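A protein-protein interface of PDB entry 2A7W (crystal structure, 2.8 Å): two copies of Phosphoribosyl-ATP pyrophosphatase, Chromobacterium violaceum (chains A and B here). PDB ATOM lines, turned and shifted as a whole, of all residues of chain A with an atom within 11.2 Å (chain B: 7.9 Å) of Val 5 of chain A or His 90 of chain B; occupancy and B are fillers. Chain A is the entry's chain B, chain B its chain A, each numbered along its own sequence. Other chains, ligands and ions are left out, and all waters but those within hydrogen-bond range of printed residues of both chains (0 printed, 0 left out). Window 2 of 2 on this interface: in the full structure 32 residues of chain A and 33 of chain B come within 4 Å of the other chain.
OE2 of Glu 88 of chain B lies within salt-bridge range of NH2 of Arg 62 of chain A, 3.0 Å away.
NH2 of Arg 92 of chain B lies within hydrogen-bond range of O of Arg 62 of chain A (2.8 Å).
NH1 of Arg 92 of chain B lies within salt-bridge range of OD1 of Asp 66 of chain A.
NE of Arg 92 of chain B lies within salt-bridge range of OE2 of Glu 88 of chain B (3.2 Å).
The backbone NH of Val 5 of chain A sits close to the side-chain amide nitrogen of Asn 8 of chain A, 3.3 Å away.
Among the printed residues, pairs that only touch across the chains: Ala 65 of chain A with Val 85 of chain B, Phe 69 of chain A with Glu 93 of chain B, Ala 65 of chain A with Leu 89 of chain B, Val 64 of chain A with Val 85 of chain B, Ala 65 of chain A with Glu 88 of chain B, Val 5 of chain A with His 90 of chain B, Leu 6 of chain A with Leu 89 of chain B, Val 61 of chain A with Asp 84 of chain B, Ala 65 of chain A with Arg 92 of chain B, Phe 69 of chain A with Leu 89 of chain B and Val 5 of chain A with Val 86 of chain B.
Printed residues of chain B within 4 Å of Val 5 of chain A: Val 86 and His 90.
His 90 of chain B touches just one residue of chain A: Val 5 (3.8 Å).
No residue of chain B comes within 4 Å of Asp 4 of chain A.
Of chain A, only Arg 62 and Ala 65 come within 4 Å of Glu 88 of chain B.
Leu 89 of chain B touches three residues of chain A.
Gly 94 of chain B touches none of the printed residues of chain A.
Printed residues of chain B within 4 Å of Val 64 of chain A: Val 85.
Of the printed residues of chain A, Glu 93 of chain B touches Phe 69.
The nearest printed residue of chain B that does not touch Val 5 of chain A is Leu 89 of chain B (5.1 Å).
The nearest printed residue of chain B that does not touch Val 64 of chain A is Leu 89 of chain B (6.2 Å).
Printed residues of chain B that touch a printed residue of chain A: Asp 84, Val 85, Val 86, Glu 88, Leu 89, His 90, Arg 92 and Glu 93.
Of the 23 printed residues of chain A, 8 touch a printed residue of chain B.
Hydrophobic or aromatic side chains of chain A within 4 Å of the printed part of chain B: Val 5, Leu 6, Val 61, Val 64, Ala 65 and Phe 69.
Along chain A the printed residues that touch a printed residue of chain B span positions 5 to 69.
Among the printed residues, 14 pairs touch across the chains.
Among the printed residues, Asp or Glu carboxylates within 4 Å of a Lys or Arg side-chain nitrogen of the other chain: Arg 62 of chain A with Glu 88 of chain B and Asp 66 of chain A with Arg 92 of chain B.
Positions printed for both chains: 83 and 86.
Of the 14 pairs that touch across the chains among the printed residues, none has its exchanged pair printed and touching as well.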
ATOM      1  N   ASP A   4       5.220 -12.802 -21.539  1.00  0.00           N
ATOM      2  CA  ASP A   4       4.647 -12.396 -20.227  1.00  0.00           C
ATOM      3  C   ASP A   4       4.537 -13.584 -19.264  1.00  0.00           C
ATOM      4  O   ASP A   4       5.430 -13.799 -18.444  1.00  0.00           O
ATOM      5  CB  ASP A   4       3.289 -11.682 -20.421  1.00  0.00           C
ATOM      6  CG  ASP A   4       2.258 -12.527 -21.184  1.00  0.00           C
ATOM      7  OD1 ASP A   4       2.592 -13.112 -22.233  1.00  0.00           O
ATOM      8  OD2 ASP A   4       1.093 -12.592 -20.734  1.00  0.00           O
ATOM      9  N   VAL A   5       3.452 -14.347 -19.382  1.00  0.00           N
ATOM     10  CA  VAL A   5       3.181 -15.527 -18.552  1.00  0.00           C
ATOM     11  C   VAL A   5       2.678 -16.618 -19.493  1.00  0.00           C
ATOM     12  O   VAL A   5       3.061 -17.786 -19.388  1.00  0.00           O
ATOM     13  CB  VAL A   5       2.059 -15.255 -17.522  1.00  0.00           C
ATOM     14  CG1 VAL A   5       1.877 -16.459 -16.616  1.00  0.00           C
ATOM     15  CG2 VAL A   5       2.362 -14.003 -16.713  1.00  0.00           C
ATOM     16  N   LEU A   6       1.806 -16.203 -20.410  1.00  0.00           N
ATOM     17  CA  LEU A   6       1.209 -17.076 -21.413  1.00  0.00           C
ATOM     18  C   LEU A   6       2.284 -17.503 -22.400  1.00  0.00           C
ATOM     19  O   LEU A   6       2.328 -18.658 -22.816  1.00  0.00           O
ATOM     20  CB  LEU A   6       0.076 -16.339 -22.150  1.00  0.00           C
ATOM     21  CG  LEU A   6      -1.025 -15.667 -21.310  1.00  0.00           C
ATOM     22  CD1 LEU A   6      -1.999 -14.908 -22.171  1.00  0.00           C
ATOM     23  CD2 LEU A   6      -1.755 -16.698 -20.482  1.00  0.00           C
ATOM     24  N   LYS A   7       3.163 -16.564 -22.742  1.00  0.00           N
ATOM     25  CA  LYS A   7       4.259 -16.822 -23.673  1.00  0.00           C
ATOM     26  C   LYS A   7       5.135 -17.958 -23.173  1.00  0.00           C
ATOM     27  O   LYS A   7       5.519 -18.848 -23.932  1.00  0.00           O
ATOM     28  CB  LYS A   7       5.117 -15.566 -23.871  1.00  0.00           C
ATOM     29  CG  LYS A   7       4.422 -14.443 -24.629  1.00  0.00           C
ATOM     30  CD  LYS A   7       5.403 -13.359 -25.068  1.00  0.00           C
ATOM     31  CE  LYS A   7       4.706 -12.293 -25.901  1.00  0.00           C
ATOM     32  NZ  LYS A   7       5.674 -11.342 -26.500  1.00  0.00           N
ATOM     33  N   ASN A   8       5.424 -17.925 -21.880  1.00  0.00           N
ATOM     34  CA  ASN A   8       6.260 -18.933 -21.245  1.00  0.00           C
ATOM     35  C   ASN A   8       5.570 -20.276 -21.294  1.00  0.00           C
ATOM     36  O   ASN A   8       6.195 -21.287 -21.598  1.00  0.00           O
ATOM     37  CB  ASN A   8       6.562 -18.525 -19.809  1.00  0.00           C
ATOM     38  CG  ASN A   8       7.100 -17.110 -19.721  1.00  0.00           C
ATOM     39  OD1 ASN A   8       8.288 -16.908 -19.487  1.00  0.00           O
ATOM     40  ND2 ASN A   8       6.233 -16.121 -19.959  1.00  0.00           N
ATOM     41  N   ILE A   9       4.267 -20.271 -21.027  1.00  0.00           N
ATOM     42  CA  ILE A   9       3.464 -21.492 -21.060  1.00  0.00           C
ATOM     43  C   ILE A   9       3.456 -22.036 -22.488  1.00  0.00           C
ATOM     44  O   ILE A   9       3.665 -23.227 -22.709  1.00  0.00           O
ATOM     45  CB  ILE A   9       2.016 -21.221 -20.586  1.00  0.00           C
ATOM     46  CG1 ILE A   9       2.023 -20.808 -19.109  1.00  0.00           C
ATOM     47  CG2 ILE A   9       1.141 -22.450 -20.801  1.00  0.00           C
ATOM     48  CD1 ILE A   9       0.654 -20.461 -18.549  1.00  0.00           C
ATOM     49  N   ALA A  10       3.263 -21.138 -23.453  1.00  0.00           N
ATOM     50  CA  ALA A  10       3.251 -21.499 -24.869  1.00  0.00           C
ATOM     51  C   ALA A  10       4.561 -22.164 -25.258  1.00  0.00           C
ATOM     52  O   ALA A  10       4.564 -23.246 -25.841  1.00  0.00           O
ATOM     53  CB  ALA A  10       3.025 -20.264 -25.727  1.00  0.00           C
ATOM     54  N   ASP A  11       5.669 -21.507 -24.911  1.00  0.00           N
ATOM     55  CA  ASP A  11       7.011 -22.013 -25.204  1.00  0.00           C
ATOM     56  C   ASP A  11       7.211 -23.392 -24.592  1.00  0.00           C
ATOM     57  O   ASP A  11       7.815 -24.267 -25.208  1.00  0.00           O
ATOM     58  CB  ASP A  11       8.097 -21.055 -24.682  1.00  0.00           C
ATOM     59  CG  ASP A  11       8.091 -19.702 -25.390  1.00  0.00           C
ATOM     60  OD1 ASP A  11       7.631 -19.620 -26.546  1.00  0.00           O
ATOM     61  OD2 ASP A  11       8.561 -18.709 -24.787  1.00  0.00           O
ATOM     62  N   THR A  12       6.683 -23.579 -23.386  1.00  0.00           N
ATOM     63  CA  THR A  12       6.795 -24.851 -22.679  1.00  0.00           C
ATOM     64  C   THR A  12       6.005 -25.924 -23.420  1.00  0.00           C
ATOM     65  O   THR A  12       6.445 -27.077 -23.521  1.00  0.00           O
ATOM     66  CB  THR A  12       6.263 -24.750 -21.240  1.00  0.00           C
ATOM     67  OG1 THR A  12       6.868 -23.631 -20.586  1.00  0.00           O
ATOM     68  CG2 THR A  12       6.606 -26.009 -20.466  1.00  0.00           C
ATOM     69  N   LEU A  13       4.841 -25.533 -23.941  1.00  0.00           N
ATOM     70  CA  LEU A  13       3.979 -26.450 -24.684  1.00  0.00           C
ATOM     71  C   LEU A  13       4.688 -26.893 -25.960  1.00  0.00           C
ATOM     72  O   LEU A  13       4.820 -28.091 -26.223  1.00  0.00           O
ATOM     73  CB  LEU A  13       2.641 -25.784 -25.024  1.00  0.00           C
ATOM     74  CG  LEU A  13       1.752 -25.375 -23.847  1.00  0.00           C
ATOM     75  CD1 LEU A  13       0.592 -24.536 -24.337  1.00  0.00           C
ATOM     76  CD2 LEU A  13       1.263 -26.599 -23.113  1.00  0.00           C
ATOM     77  N   GLU A  14       5.173 -25.915 -26.723  1.00  0.00           N
ATOM     78  CA  GLU A  14       5.884 -26.188 -27.964  1.00  0.00           C
ATOM     79  C   GLU A  14       7.112 -27.039 -27.693  1.00  0.00           C
ATOM     80  O   GLU A  14       7.463 -27.908 -28.488  1.00  0.00           O
ATOM     81  CB  GLU A  14       6.307 -24.888 -28.641  1.00  0.00           C
ATOM     82  CG  GLU A  14       5.151 -23.998 -29.055  1.00  0.00           C
ATOM     83  CD  GLU A  14       5.593 -22.736 -29.780  1.00  0.00           C
ATOM     84  OE1 GLU A  14       6.728 -22.262 -29.557  1.00  0.00           O
ATOM     85  OE2 GLU A  14       4.791 -22.205 -30.573  1.00  0.00           O
ATOM     86  N   VAL A  61     -12.776 -19.356 -11.602  1.00  0.00           N
ATOM     87  CA  VAL A  61     -11.454 -18.941 -12.033  1.00  0.00           C
ATOM     88  C   VAL A  61     -10.552 -20.135 -12.326  1.00  0.00           C
ATOM     89  O   VAL A  61      -9.787 -20.112 -13.276  1.00  0.00           O
ATOM     90  CB  VAL A  61     -10.794 -18.016 -10.989  1.00  0.00           C
ATOM     91  CG1 VAL A  61      -9.352 -17.714 -11.378  1.00  0.00           C
ATOM     92  CG2 VAL A  61     -11.595 -16.725 -10.847  1.00  0.00           C
ATOM     93  N   ARG A  62     -10.649 -21.188 -11.533  1.00  0.00           N
ATOM     94  CA  ARG A  62      -9.814 -22.356 -11.776  1.00  0.00           C
ATOM     95  C   ARG A  62     -10.179 -23.011 -13.102  1.00  0.00           C
ATOM     96  O   ARG A  62      -9.304 -23.454 -13.839  1.00  0.00           O
ATOM     97  CB  ARG A  62      -9.946 -23.388 -10.653  1.00  0.00           C
ATOM     98  CG  ARG A  62      -9.597 -22.863  -9.268  1.00  0.00           C
ATOM     99  CD  ARG A  62      -8.854 -23.905  -8.451  1.00  0.00           C
ATOM    100  NE  ARG A  62      -7.467 -24.049  -8.893  1.00  0.00           N
ATOM    101  CZ  ARG A  62      -6.723 -25.143  -8.724  1.00  0.00           C
ATOM    102  NH1 ARG A  62      -7.225 -26.214  -8.122  1.00  0.00           N
ATOM    103  NH2 ARG A  62      -5.463 -25.163  -9.141  1.00  0.00           N
ATOM    104  N   VAL A  64     -11.951 -21.525 -15.794  1.00  0.00           N
ATOM    105  CA  VAL A  64     -11.669 -20.619 -16.898  1.00  0.00           C
ATOM    106  C   VAL A  64     -10.179 -20.716 -17.239  1.00  0.00           C
ATOM    107  O   VAL A  64      -9.793 -20.680 -18.412  1.00  0.00           O
ATOM    108  CB  VAL A  64     -12.023 -19.173 -16.556  1.00  0.00           C
ATOM    109  CG1 VAL A  64     -11.400 -18.246 -17.553  1.00  0.00           C
ATOM    110  CG2 VAL A  64     -13.527 -18.982 -16.569  1.00  0.00           C
ATOM    111  N   ALA A  65      -9.357 -20.914 -16.216  1.00  0.00           N
ATOM    112  CA  ALA A  65      -7.927 -21.041 -16.414  1.00  0.00           C
ATOM    113  C   ALA A  65      -7.601 -22.346 -17.097  1.00  0.00           C
ATOM    114  O   ALA A  65      -6.772 -22.412 -17.995  1.00  0.00           O
ATOM    115  CB  ALA A  65      -7.208 -20.953 -15.088  1.00  0.00           C
ATOM    116  N   ASP A  66      -8.260 -23.399 -16.656  1.00  0.00           N
ATOM    117  CA  ASP A  66      -8.035 -24.716 -17.230  1.00  0.00           C
ATOM    118  C   ASP A  66      -8.502 -24.727 -18.691  1.00  0.00           C
ATOM    119  O   ASP A  66      -7.912 -25.398 -19.530  1.00  0.00           O
ATOM    120  CB  ASP A  66      -8.764 -25.775 -16.399  1.00  0.00           C
ATOM    121  CG  ASP A  66      -8.026 -27.104 -16.365  1.00  0.00           C
ATOM    122  OD1 ASP A  66      -6.833 -27.138 -16.760  1.00  0.00           O
ATOM    123  OD2 ASP A  66      -8.634 -28.120 -15.939  1.00  0.00           O
ATOM    124  N   TRP A  68      -8.622 -21.922 -20.781  1.00  0.00           N
ATOM    125  CA  TRP A  68      -7.608 -21.195 -21.546  1.00  0.00           C
ATOM    126  C   TRP A  68      -6.394 -22.073 -21.753  1.00  0.00           C
ATOM    127  O   TRP A  68      -5.853 -22.149 -22.848  1.00  0.00           O
ATOM    128  CB  TRP A  68      -7.169 -19.921 -20.849  1.00  0.00           C
ATOM    129  CG  TRP A  68      -8.158 -18.849 -20.869  1.00  0.00           C
ATOM    130  CD1 TRP A  68      -9.509 -18.971 -20.983  1.00  0.00           C
ATOM    131  CD2 TRP A  68      -7.892 -17.464 -20.678  1.00  0.00           C
ATOM    132  NE1 TRP A  68     -10.107 -17.733 -20.858  1.00  0.00           N
ATOM    133  CE2 TRP A  68      -9.130 -16.793 -20.671  1.00  0.00           C
ATOM    134  CE3 TRP A  68      -6.717 -16.725 -20.502  1.00  0.00           C
ATOM    135  CZ2 TRP A  68      -9.236 -15.420 -20.495  1.00  0.00           C
ATOM    136  CZ3 TRP A  68      -6.818 -15.346 -20.320  1.00  0.00           C
ATOM    137  CH2 TRP A  68      -8.073 -14.709 -20.320  1.00  0.00           C
ATOM    138  N   PHE A  69      -5.987 -22.777 -20.714  1.00  0.00           N
ATOM    139  CA  PHE A  69      -4.828 -23.643 -20.836  1.00  0.00           C
ATOM    140  C   PHE A  69      -4.995 -24.670 -21.939  1.00  0.00           C
ATOM    141  O   PHE A  69      -4.114 -24.834 -22.763  1.00  0.00           O
ATOM    142  CB  PHE A  69      -4.515 -24.370 -19.523  1.00  0.00           C
ATOM    143  CG  PHE A  69      -3.330 -25.298 -19.624  1.00  0.00           C
ATOM    144  CD1 PHE A  69      -2.041 -24.791 -19.731  1.00  0.00           C
ATOM    145  CD2 PHE A  69      -3.497 -26.680 -19.644  1.00  0.00           C
ATOM    146  CE1 PHE A  69      -0.935 -25.657 -19.858  1.00  0.00           C
ATOM    147  CE2 PHE A  69      -2.391 -27.545 -19.771  1.00  0.00           C
ATOM    148  CZ  PHE A  69      -1.116 -27.028 -19.879  1.00  0.00           C
ATOM    149  N   MET A  72      -4.869 -23.255 -25.319  1.00  0.00           N
ATOM    150  CA  MET A  72      -3.479 -23.029 -25.726  1.00  0.00           C
ATOM    151  C   MET A  72      -2.836 -24.345 -26.172  1.00  0.00           C
ATOM    152  O   MET A  72      -1.978 -24.363 -27.055  1.00  0.00           O
ATOM    153  CB  MET A  72      -2.652 -22.448 -24.577  1.00  0.00           C
ATOM    154  CG  MET A  72      -2.913 -20.995 -24.270  1.00  0.00           C
ATOM    155  SD  MET A  72      -1.679 -20.341 -23.121  1.00  0.00           S
ATOM    156  CE  MET A  72      -2.727 -19.248 -22.311  1.00  0.00           C
ATOM    157  N   ARG A  81      -0.177 -20.125 -31.712  1.00  0.00           N
ATOM    158  CA  ARG A  81       0.154 -19.770 -30.341  1.00  0.00           C
ATOM    159  C   ARG A  81      -0.591 -18.570 -29.765  1.00  0.00           C
ATOM    160  O   ARG A  81      -1.097 -17.737 -30.505  1.00  0.00           O
ATOM    161  CB  ARG A  81       1.667 -19.643 -30.153  1.00  0.00           C
ATOM    162  CG  ARG A  81       2.406 -18.759 -31.109  1.00  0.00           C
ATOM    163  CD  ARG A  81       3.881 -18.793 -30.737  1.00  0.00           C
ATOM    164  NE  ARG A  81       4.116 -18.197 -29.420  1.00  0.00           N
ATOM    165  CZ  ARG A  81       4.882 -18.724 -28.467  1.00  0.00           C
ATOM    166  NH1 ARG A  81       5.507 -19.875 -28.666  1.00  0.00           N
ATOM    167  NH2 ARG A  81       5.021 -18.096 -27.309  1.00  0.00           N
ATOM    168  N   PRO A  82      -0.664 -18.476 -28.422  1.00  0.00           N
ATOM    169  CA  PRO A  82      -1.326 -17.436 -27.631  1.00  0.00           C
ATOM    170  C   PRO A  82      -1.368 -16.044 -28.213  1.00  0.00           C
ATOM    171  O   PRO A  82      -2.434 -15.435 -28.308  1.00  0.00           O
ATOM    172  CB  PRO A  82      -0.530 -17.453 -26.336  1.00  0.00           C
ATOM    173  CG  PRO A  82      -0.338 -18.876 -26.137  1.00  0.00           C
ATOM    174  CD  PRO A  82       0.073 -19.377 -27.515  1.00  0.00           C
ATOM    175  N   GLU A  83      -0.196 -15.528 -28.558  1.00  0.00           N
ATOM    176  CA  GLU A  83      -0.070 -14.185 -29.120  1.00  0.00           C
ATOM    177  C   GLU A  83      -1.063 -13.940 -30.252  1.00  0.00           C
ATOM    178  O   GLU A  83      -1.626 -12.850 -30.360  1.00  0.00           O
ATOM    179  CB  GLU A  83       1.363 -13.934 -29.598  1.00  0.00           C
ATOM    180  CG  GLU A  83       2.414 -13.959 -28.475  1.00  0.00           C
ATOM    181  CD  GLU A  83       2.992 -15.351 -28.188  1.00  0.00           C
ATOM    182  OE1 GLU A  83       2.281 -16.367 -28.353  1.00  0.00           O
ATOM    183  OE2 GLU A  83       4.178 -15.421 -27.797  1.00  0.00           O
ATOM    184  N   VAL A  86      -4.215 -13.205 -28.578  1.00  0.00           N
ATOM    185  CA  VAL A  86      -4.107 -11.921 -27.907  1.00  0.00           C
ATOM    186  C   VAL A  86      -4.174 -10.791 -28.930  1.00  0.00           C
ATOM    187  O   VAL A  86      -4.932  -9.837 -28.753  1.00  0.00           O
ATOM    188  CB  VAL A  86      -2.811 -11.814 -27.097  1.00  0.00           C
ATOM    189  CG1 VAL A  86      -2.826 -10.537 -26.274  1.00  0.00           C
ATOM    190  CG2 VAL A  86      -2.661 -13.041 -26.196  1.00  0.00           C
ATOM    191  N   GLU B  83      -6.590 -11.023 -14.788  1.00  0.00           N
ATOM    192  CA  GLU B  83      -5.385 -11.246 -13.992  1.00  0.00           C
ATOM    193  C   GLU B  83      -5.537 -12.444 -13.066  1.00  0.00           C
ATOM    194  O   GLU B  83      -4.590 -13.207 -12.881  1.00  0.00           O
ATOM    195  CB  GLU B  83      -5.004  -9.987 -13.207  1.00  0.00           C
ATOM    196  CG  GLU B  83      -4.650  -8.773 -14.082  1.00  0.00           C
ATOM    197  CD  GLU B  83      -5.852  -7.898 -14.446  1.00  0.00           C
ATOM    198  OE1 GLU B  83      -6.962  -8.424 -14.666  1.00  0.00           O
ATOM    199  OE2 GLU B  83      -5.682  -6.663 -14.509  1.00  0.00           O
ATOM    200  N   ASP B  84      -6.741 -12.630 -12.530  1.00  0.00           N
ATOM    201  CA  ASP B  84      -7.022 -13.753 -11.653  1.00  0.00           C
ATOM    202  C   ASP B  84      -6.714 -15.037 -12.396  1.00  0.00           C
ATOM    203  O   ASP B  84      -6.000 -15.896 -11.892  1.00  0.00           O
ATOM    204  CB  ASP B  84      -8.489 -13.756 -11.208  1.00  0.00           C
ATOM    205  CG  ASP B  84      -8.851 -12.568 -10.316  1.00  0.00           C
ATOM    206  OD1 ASP B  84      -8.076 -12.237  -9.410  1.00  0.00           O
ATOM    207  OD2 ASP B  84      -9.932 -11.981 -10.513  1.00  0.00           O
ATOM    208  N   VAL B  85      -7.215 -15.133 -13.624  1.00  0.00           N
ATOM    209  CA  VAL B  85      -6.994 -16.311 -14.463  1.00  0.00           C
ATOM    210  C   VAL B  85      -5.528 -16.448 -14.859  1.00  0.00           C
ATOM    211  O   VAL B  85      -4.974 -17.548 -14.857  1.00  0.00           O
ATOM    212  CB  VAL B  85      -7.848 -16.270 -15.738  1.00  0.00           C
ATOM    213  CG1 VAL B  85      -7.620 -17.525 -16.567  1.00  0.00           C
ATOM    214  CG2 VAL B  85      -9.304 -16.119 -15.384  1.00  0.00           C
ATOM    215  N   VAL B  86      -4.906 -15.325 -15.196  1.00  0.00           N
ATOM    216  CA  VAL B  86      -3.504 -15.336 -15.582  1.00  0.00           C
ATOM    217  C   VAL B  86      -2.639 -15.782 -14.407  1.00  0.00           C
ATOM    218  O   VAL B  86      -1.782 -16.652 -14.558  1.00  0.00           O
ATOM    219  CB  VAL B  86      -3.051 -13.965 -16.084  1.00  0.00           C
ATOM    220  CG1 VAL B  86      -1.652 -14.059 -16.679  1.00  0.00           C
ATOM    221  CG2 VAL B  86      -4.050 -13.444 -17.105  1.00  0.00           C
ATOM    222  N   MET B  87      -2.889 -15.215 -13.232  1.00  0.00           N
ATOM    223  CA  MET B  87      -2.120 -15.596 -12.053  1.00  0.00           C
ATOM    224  C   MET B  87      -2.394 -17.042 -11.681  1.00  0.00           C
ATOM    225  O   MET B  87      -1.484 -17.760 -11.269  1.00  0.00           O
ATOM    226  CB  MET B  87      -2.377 -14.658 -10.877  1.00  0.00           C
ATOM    227  CG  MET B  87      -1.513 -13.409 -10.939  1.00  0.00           C
ATOM    228  SD  MET B  87      -1.741 -12.326  -9.565  1.00  0.00           S
ATOM    229  CE  MET B  87      -3.001 -11.135 -10.150  1.00  0.00           C
ATOM    230  N   GLU B  88      -3.641 -17.479 -11.855  1.00  0.00           N
ATOM    231  CA  GLU B  88      -4.000 -18.864 -11.570  1.00  0.00           C
ATOM    232  C   GLU B  88      -3.226 -19.772 -12.535  1.00  0.00           C
ATOM    233  O   GLU B  88      -2.796 -20.860 -12.164  1.00  0.00           O
ATOM    234  CB  GLU B  88      -5.514 -19.065 -11.705  1.00  0.00           C
ATOM    235  CG  GLU B  88      -5.996 -20.514 -11.589  1.00  0.00           C
ATOM    236  CD  GLU B  88      -5.485 -21.230 -10.347  1.00  0.00           C
ATOM    237  OE1 GLU B  88      -5.386 -20.602  -9.275  1.00  0.00           O
ATOM    238  OE2 GLU B  88      -5.183 -22.435 -10.439  1.00  0.00           O
ATOM    239  N   LEU B  89      -3.018 -19.295 -13.759  1.00  0.00           N
ATOM    240  CA  LEU B  89      -2.273 -20.044 -14.751  1.00  0.00           C
ATOM    241  C   LEU B  89      -0.809 -20.108 -14.346  1.00  0.00           C
ATOM    242  O   LEU B  89      -0.163 -21.147 -14.482  1.00  0.00           O
ATOM    243  CB  LEU B  89      -2.410 -19.390 -16.119  1.00  0.00           C
ATOM    244  CG  LEU B  89      -3.598 -19.832 -16.967  1.00  0.00           C
ATOM    245  CD1 LEU B  89      -3.838 -18.830 -18.076  1.00  0.00           C
ATOM    246  CD2 LEU B  89      -3.332 -21.217 -17.525  1.00  0.00           C
ATOM    247  N   HIS B  90      -0.303 -18.994 -13.826  1.00  0.00           N
ATOM    248  CA  HIS B  90       1.083 -18.897 -13.392  1.00  0.00           C
ATOM    249  C   HIS B  90       1.334 -19.797 -12.198  1.00  0.00           C
ATOM    250  O   HIS B  90       2.344 -20.499 -12.141  1.00  0.00           O
ATOM    251  CB  HIS B  90       1.415 -17.449 -13.028  1.00  0.00           C
ATOM    252  CG  HIS B  90       2.846 -17.237 -12.625  1.00  0.00           C
ATOM    253  ND1 HIS B  90       3.270 -16.080 -12.001  1.00  0.00           N
ATOM    254  CD2 HIS B  90       3.936 -18.020 -12.756  1.00  0.00           C
ATOM    255  CE1 HIS B  90       4.567 -16.168 -11.766  1.00  0.00           C
ATOM    256  NE2 HIS B  90       5.000 -17.332 -12.212  1.00  0.00           N
ATOM    257  N   ARG B  91       0.400 -19.780 -11.251  1.00  0.00           N
ATOM    258  CA  ARG B  91       0.506 -20.586 -10.042  1.00  0.00           C
ATOM    259  C   ARG B  91       0.686 -22.068 -10.371  1.00  0.00           C
ATOM    260  O   ARG B  91       1.381 -22.784  -9.656  1.00  0.00           O
ATOM    261  CB  ARG B  91      -0.730 -20.384  -9.171  1.00  0.00           C
ATOM    262  CG  ARG B  91      -0.527 -20.815  -7.744  1.00  0.00           C
ATOM    263  CD  ARG B  91      -1.840 -20.977  -7.007  1.00  0.00           C
ATOM    264  NE  ARG B  91      -1.611 -21.506  -5.669  1.00  0.00           N
ATOM    265  CZ  ARG B  91      -1.145 -22.726  -5.416  1.00  0.00           C
ATOM    266  NH1 ARG B  91      -0.864 -23.556  -6.411  1.00  0.00           N
ATOM    267  NH2 ARG B  91      -0.915 -23.106  -4.168  1.00  0.00           N
ATOM    268  N   ARG B  92       0.078 -22.512 -11.469  1.00  0.00           N
ATOM    269  CA  ARG B  92       0.181 -23.901 -11.905  1.00  0.00           C
ATOM    270  C   ARG B  92       1.521 -24.161 -12.596  1.00  0.00           C
ATOM    271  O   ARG B  92       2.490 -24.566 -11.951  1.00  0.00           O
ATOM    272  CB  ARG B  92      -0.957 -24.238 -12.866  1.00  0.00           C
ATOM    273  CG  ARG B  92      -2.342 -24.178 -12.268  1.00  0.00           C
ATOM    274  CD  ARG B  92      -3.370 -24.458 -13.341  1.00  0.00           C
ATOM    275  NE  ARG B  92      -4.730 -24.520 -12.822  1.00  0.00           N
ATOM    276  CZ  ARG B  92      -5.804 -24.739 -13.574  1.00  0.00           C
ATOM    277  NH1 ARG B  92      -5.676 -24.917 -14.882  1.00  0.00           N
ATOM    278  NH2 ARG B  92      -7.007 -24.781 -13.020  1.00  0.00           N
ATOM    279  N   GLU B  93       1.561 -23.926 -13.910  1.00  0.00           N
ATOM    280  CA  GLU B  93       2.771 -24.124 -14.720  1.00  0.00           C
ATOM    281  C   GLU B  93       3.838 -23.069 -14.420  1.00  0.00           C
ATOM    282  O   GLU B  93       3.660 -21.886 -14.720  1.00  0.00           O
ATOM    283  CB  GLU B  93       2.442 -24.115 -16.225  1.00  0.00           C
ATOM    284  CG  GLU B  93       1.853 -25.421 -16.783  1.00  0.00           C
ATOM    285  CD  GLU B  93       0.400 -25.661 -16.385  1.00  0.00           C
ATOM    286  OE1 GLU B  93      -0.405 -24.703 -16.448  1.00  0.00           O
ATOM    287  OE2 GLU B  93       0.059 -26.815 -16.029  1.00  0.00           O
ATOM    288  N   GLY B  94       4.947 -23.517 -13.837  1.00  0.00           N
ATOM    289  CA  GLY B  94       6.036 -22.619 -13.492  1.00  0.00           C
ATOM    290  C   GLY B  94       5.942 -22.114 -12.064  1.00  0.00           C
ATOM    291  O   GLY B  94       6.130 -22.923 -11.128  1.00  0.00           O
